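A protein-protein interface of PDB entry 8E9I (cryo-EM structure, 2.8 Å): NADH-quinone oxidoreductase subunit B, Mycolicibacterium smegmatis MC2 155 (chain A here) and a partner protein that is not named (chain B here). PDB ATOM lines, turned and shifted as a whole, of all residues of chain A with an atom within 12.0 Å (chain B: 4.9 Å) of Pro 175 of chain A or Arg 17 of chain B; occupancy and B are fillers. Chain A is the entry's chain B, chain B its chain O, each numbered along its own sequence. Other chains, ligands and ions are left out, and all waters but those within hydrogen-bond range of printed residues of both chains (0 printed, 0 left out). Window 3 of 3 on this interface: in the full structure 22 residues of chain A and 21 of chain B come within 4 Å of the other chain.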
ATOM      1  N   ALA A 169       6.286   8.730  16.500  1.00  0.00           N
ATOM      2  CA  ALA A 169       6.093   8.429  17.913  1.00  0.00           C
ATOM      3  C   ALA A 169       7.089   9.192  18.773  1.00  0.00           C
ATOM      4  O   ALA A 169       6.739   9.716  19.835  1.00  0.00           O
ATOM      5  CB  ALA A 169       6.222   6.925  18.148  1.00  0.00           C
ATOM      6  N   ALA A 170       8.343   9.268  18.324  1.00  0.00           N
ATOM      7  CA  ALA A 170       9.387   9.882  19.134  1.00  0.00           C
ATOM      8  C   ALA A 170       9.166  11.376  19.308  1.00  0.00           C
ATOM      9  O   ALA A 170       9.609  11.954  20.304  1.00  0.00           O
ATOM     10  CB  ALA A 170      10.754   9.628  18.502  1.00  0.00           C
ATOM     11  N   LEU A 171       8.499  12.018  18.353  1.00  0.00           N
ATOM     12  CA  LEU A 171       8.327  13.462  18.426  1.00  0.00           C
ATOM     13  C   LEU A 171       7.420  13.866  19.579  1.00  0.00           C
ATOM     14  O   LEU A 171       7.406  15.036  19.976  1.00  0.00           O
ATOM     15  CB  LEU A 171       7.766  13.981  17.105  1.00  0.00           C
ATOM     16  CG  LEU A 171       8.793  14.145  15.985  1.00  0.00           C
ATOM     17  CD1 LEU A 171       8.098  14.230  14.639  1.00  0.00           C
ATOM     18  CD2 LEU A 171       9.654  15.362  16.221  1.00  0.00           C
ATOM     19  N   ALA A 172       6.664  12.922  20.134  1.00  0.00           N
ATOM     20  CA  ALA A 172       5.645  13.245  21.121  1.00  0.00           C
ATOM     21  C   ALA A 172       6.082  13.008  22.561  1.00  0.00           C
ATOM     22  O   ALA A 172       5.553  13.668  23.463  1.00  0.00           O
ATOM     23  CB  ALA A 172       4.381  12.430  20.848  1.00  0.00           C
ATOM     24  N   VAL A 173       7.023  12.103  22.802  1.00  0.00           N
ATOM     25  CA  VAL A 173       7.381  11.764  24.186  1.00  0.00           C
ATOM     26  C   VAL A 173       7.888  13.014  24.895  1.00  0.00           C
ATOM     27  O   VAL A 173       8.816  13.669  24.392  1.00  0.00           O
ATOM     28  CB  VAL A 173       8.438  10.656  24.211  1.00  0.00           C
ATOM     29  CG1 VAL A 173       7.897   9.383  23.578  1.00  0.00           C
ATOM     30  CG2 VAL A 173       9.716  11.112  23.512  1.00  0.00           C
ATOM     31  N   PRO A 174       7.326  13.394  26.041  1.00  0.00           N
ATOM     32  CA  PRO A 174       7.885  14.521  26.774  1.00  0.00           C
ATOM     33  C   PRO A 174       9.247  14.163  27.329  1.00  0.00           C
ATOM     34  O   PRO A 174       9.497  13.002  27.704  1.00  0.00           O
ATOM     35  CB  PRO A 174       6.859  14.760  27.890  1.00  0.00           C
ATOM     36  CG  PRO A 174       6.230  13.440  28.105  1.00  0.00           C
ATOM     37  CD  PRO A 174       6.202  12.771  26.762  1.00  0.00           C
ATOM     38  N   PRO A 175      10.159  15.127  27.413  1.00  0.00           N
ATOM     39  CA  PRO A 175      11.521  14.808  27.846  1.00  0.00           C
ATOM     40  C   PRO A 175      11.549  14.374  29.303  1.00  0.00           C
ATOM     41  O   PRO A 175      10.690  14.735  30.107  1.00  0.00           O
ATOM     42  CB  PRO A 175      12.275  16.123  27.636  1.00  0.00           C
ATOM     43  CG  PRO A 175      11.242  17.165  27.814  1.00  0.00           C
ATOM     44  CD  PRO A 175       9.941  16.580  27.324  1.00  0.00           C
ATOM     45  N   THR A 176      12.568  13.579  29.632  1.00  0.00           N
ATOM     46  CA  THR A 176      12.667  13.024  30.977  1.00  0.00           C
ATOM     47  C   THR A 176      12.553  14.109  32.036  1.00  0.00           C
ATOM     48  O   THR A 176      11.921  13.906  33.078  1.00  0.00           O
ATOM     49  CB  THR A 176      13.985  12.270  31.141  1.00  0.00           C
ATOM     50  OG1 THR A 176      15.080  13.155  30.880  1.00  0.00           O
ATOM     51  CG2 THR A 176      14.052  11.094  30.193  1.00  0.00           C
ATOM     52  N   ILE A 177      13.151  15.272  31.790  1.00  0.00           N
ATOM     53  CA  ILE A 177      13.129  16.352  32.760  1.00  0.00           C
ATOM     54  C   ILE A 177      11.737  16.910  32.989  1.00  0.00           C
ATOM     55  O   ILE A 177      11.533  17.653  33.951  1.00  0.00           O
ATOM     56  CB  ILE A 177      14.065  17.489  32.316  1.00  0.00           C
ATOM     57  CG1 ILE A 177      14.257  18.485  33.460  1.00  0.00           C
ATOM     58  CG2 ILE A 177      13.511  18.181  31.080  1.00  0.00           C
ATOM     59  CD1 ILE A 177      15.486  19.342  33.313  1.00  0.00           C
ATOM     60  N   GLU A 178      10.779  16.591  32.126  1.00  0.00           N
ATOM     61  CA  GLU A 178       9.418  17.082  32.275  1.00  0.00           C
ATOM     62  C   GLU A 178       8.472  16.042  32.854  1.00  0.00           C
ATOM     63  O   GLU A 178       7.297  16.349  33.067  1.00  0.00           O
ATOM     64  CB  GLU A 178       8.883  17.564  30.925  1.00  0.00           C
ATOM     65  N   LEU A 179       8.948  14.826  33.126  1.00  0.00           N
ATOM     66  CA  LEU A 179       8.094  13.792  33.699  1.00  0.00           C
ATOM     67  C   LEU A 179       7.990  13.963  35.208  1.00  0.00           C
ATOM     68  O   LEU A 179       8.215  13.013  35.965  1.00  0.00           O
ATOM     69  CB  LEU A 179       8.632  12.399  33.371  1.00  0.00           C
ATOM     70  CG  LEU A 179       8.240  11.785  32.031  1.00  0.00           C
ATOM     71  CD1 LEU A 179       8.579  12.714  30.894  1.00  0.00           C
ATOM     72  CD2 LEU A 179       8.958  10.459  31.858  1.00  0.00           C
ATOM     73  N   LYS A 180       7.641  15.166  35.655  1.00  0.00           N
ATOM     74  CA  LYS A 180       7.471  15.418  37.077  1.00  0.00           C
ATOM     75  C   LYS A 180       6.267  14.643  37.590  1.00  0.00           C
ATOM     76  O   LYS A 180       5.126  14.968  37.253  1.00  0.00           O
ATOM     77  CB  LYS A 180       7.298  16.915  37.341  1.00  0.00           C
ATOM     78  N   GLY A 181       6.509  13.623  38.408  1.00  0.00           N
ATOM     79  CA  GLY A 181       5.432  12.802  38.924  1.00  0.00           C
ATOM     80  C   GLY A 181       4.916  13.322  40.247  1.00  0.00           C
ATOM     81  O   GLY A 181       4.299  14.388  40.304  1.00  0.00           O
ATOM     82  N   LEU A 183       6.769  14.465  42.272  1.00  0.00           N
ATOM     83  CA  LEU A 183       7.873  15.345  42.634  1.00  0.00           C
ATOM     84  C   LEU A 183       7.366  16.771  42.850  1.00  0.00           C
ATOM     85  O   LEU A 183       7.812  17.729  42.224  1.00  0.00           O
ATOM     86  CB  LEU A 183       8.933  15.287  41.545  1.00  0.00           C
ATOM     87  CG  LEU A 183      10.291  15.922  41.813  1.00  0.00           C
ATOM     88  CD1 LEU A 183      10.915  15.384  43.086  1.00  0.00           C
ATOM     89  CD2 LEU A 183      11.192  15.661  40.632  1.00  0.00           C
ATOM     90  N   ASN B  15      14.636  15.693  22.494  1.00  0.00           N
ATOM     91  CA  ASN B  15      13.980  16.552  23.467  1.00  0.00           C
ATOM     92  C   ASN B  15      13.094  17.536  22.719  1.00  0.00           C
ATOM     93  O   ASN B  15      13.607  18.398  21.996  1.00  0.00           O
ATOM     94  CB  ASN B  15      15.003  17.301  24.323  1.00  0.00           C
ATOM     95  CG  ASN B  15      14.351  18.207  25.355  1.00  0.00           C
ATOM     96  OD1 ASN B  15      13.219  18.654  25.185  1.00  0.00           O
ATOM     97  ND2 ASN B  15      15.075  18.492  26.428  1.00  0.00           N
ATOM     98  N   PRO B  16      11.771  17.454  22.864  1.00  0.00           N
ATOM     99  CA  PRO B  16      10.921  18.424  22.165  1.00  0.00           C
ATOM    100  C   PRO B  16      11.215  19.854  22.563  1.00  0.00           C
ATOM    101  O   PRO B  16      11.134  20.759  21.724  1.00  0.00           O
ATOM    102  CB  PRO B  16       9.501  17.999  22.567  1.00  0.00           C
ATOM    103  CG  PRO B  16       9.630  16.603  23.035  1.00  0.00           C
ATOM    104  CD  PRO B  16      10.975  16.518  23.668  1.00  0.00           C
ATOM    105  N   ARG B  17      11.555  20.087  23.828  1.00  0.00           N
ATOM    106  CA  ARG B  17      11.768  21.454  24.279  1.00  0.00           C
ATOM    107  C   ARG B  17      13.000  22.068  23.640  1.00  0.00           C
ATOM    108  O   ARG B  17      13.006  23.264  23.351  1.00  0.00           O
ATOM    109  CB  ARG B  17      11.877  21.501  25.800  1.00  0.00           C
ATOM    110  CG  ARG B  17      10.754  20.772  26.517  1.00  0.00           C
ATOM    111  CD  ARG B  17       9.371  21.252  26.111  1.00  0.00           C
ATOM    112  NE  ARG B  17       8.345  20.338  26.598  1.00  0.00           N
ATOM    113  CZ  ARG B  17       7.394  19.790  25.851  1.00  0.00           C
ATOM    114  NH1 ARG B  17       7.251  20.091  24.571  1.00  0.00           N
ATOM    115  NH2 ARG B  17       6.559  18.916  26.405  1.00  0.00           N
ATOM    116  N   THR B  18      14.048  21.279  23.407  1.00  0.00           N
ATOM    117  CA  THR B  18      15.202  21.815  22.693  1.00  0.00           C
ATOM    118  C   THR B  18      14.835  22.180  21.262  1.00  0.00           C
ATOM    119  O   THR B  18      15.301  23.196  20.735  1.00  0.00           O
ATOM    120  CB  THR B  18      16.354  20.818  22.707  1.00  0.00           C
ATOM    121  OG1 THR B  18      15.947  19.608  22.060  1.00  0.00           O
ATOM    122  CG2 THR B  18      16.790  20.523  24.128  1.00  0.00           C
ATOM    123  N   ARG B  19      14.006  21.364  20.611  1.00  0.00           N
ATOM    124  CA  ARG B  19      13.571  21.715  19.266  1.00  0.00           C
ATOM    125  C   ARG B  19      12.766  23.004  19.276  1.00  0.00           C
ATOM    126  O   ARG B  19      12.972  23.877  18.427  1.00  0.00           O
ATOM    127  CB  ARG B  19      12.752  20.579  18.660  1.00  0.00           C
ATOM    128  CG  ARG B  19      13.455  19.236  18.657  1.00  0.00           C
ATOM    129  CD  ARG B  19      12.817  18.310  17.652  1.00  0.00           C
ATOM    130  NE  ARG B  19      11.376  18.229  17.847  1.00  0.00           N
ATOM    131  CZ  ARG B  19      10.758  17.309  18.574  1.00  0.00           C
ATOM    132  NH1 ARG B  19      11.426  16.351  19.199  1.00  0.00           N
ATOM    133  NH2 ARG B  19       9.435  17.352  18.680  1.00  0.00           N
ATOM    134  N   GLU B  20      11.846  23.144  20.230  1.00  0.00           N
ATOM    135  CA  GLU B  20      11.070  24.376  20.320  1.00  0.00           C
ATOM    136  C   GLU B  20      11.976  25.563  20.608  1.00  0.00           C
ATOM    137  O   GLU B  20      11.768  26.657  20.078  1.00  0.00           O
ATOM    138  CB  GLU B  20       9.997  24.241  21.396  1.00  0.00           C
ATOM    139  N   GLN B  21      12.987  25.366  21.448  1.00  0.00           N
ATOM    140  CA  GLN B  21      13.917  26.438  21.769  1.00  0.00           C
ATOM    141  C   GLN B  21      14.691  26.876  20.531  1.00  0.00           C
ATOM    142  O   GLN B  21      14.888  28.074  20.295  1.00  0.00           O
ATOM    143  CB  GLN B  21      14.863  25.966  22.870  1.00  0.00           C
ATOM    144  CG  GLN B  21      15.685  27.059  23.503  1.00  0.00           C
ATOM    145  CD  GLN B  21      14.998  27.689  24.687  1.00  0.00           C
ATOM    146  OE1 GLN B  21      14.017  27.160  25.204  1.00  0.00           O
ATOM    147  NE2 GLN B  21      15.509  28.831  25.128  1.00  0.00           N
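The backbone carbonyl oxygen (O) of Leu 171 of chain A sits close to the guanidinium group (NH2) of Arg 19 of chain B.
N of Arg 17 of chain B sits at hydrogen-bond distance from OD1 of Asn 15 of chain B (2.6 Å).
The side-chain hydroxyl (OG1) of Thr 18 of chain B sits at hydrogen-bond distance from the backbone carbonyl oxygen (O) of Asn 15 of chain B, at 2.6 Å.
CG of Pro 16 of chain B touches O of Val 173 of chain A, at 3.3 Å.
Asn 15 of chain B touches Pro 175 of chain A.
CD of Pro 16 of chain B touches CD of Pro 175 of chain A, 3.8 Å away.
Arg 17 of chain B touches Pro 175 of chain A (CG to CG, 3.9 Å).
Of the printed residues of chain B, Leu 171 of chain A touches Arg 19.
Ala 172 of chain A touches none of the printed residues of chain B.
Printed residues of chain B within 4 Å of Val 173 of chain A: Pro 16.
Pro 175 of chain A touches three residues of chain B.
Glu 178 of chain A touches none of the printed residues of chain B.
Printed residues of chain A within 4 Å of Asn 15 of chain B: Pro 175 (3.6 Å).
Arg 17 of chain B touches one residue of chain A.
No residue of chain A comes within 4 Å of Glu 20 of chain B.
The nearest residue of chain A that does not touch Arg 17 of chain B is Pro 174 of chain A (4.4 Å).
Hydrophobic or aromatic side chains of chain A within 4 Å of the printed part of chain B: Leu 171 and Pro 175.
Printed residues of chain B that touch a printed residue of chain A: Asn 15, Pro 16, Arg 17 and Arg 19.
Among the printed residues, no Asp or Glu carboxylate lies within 4 Å of a Lys or Arg side-chain nitrogen of the other chain.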
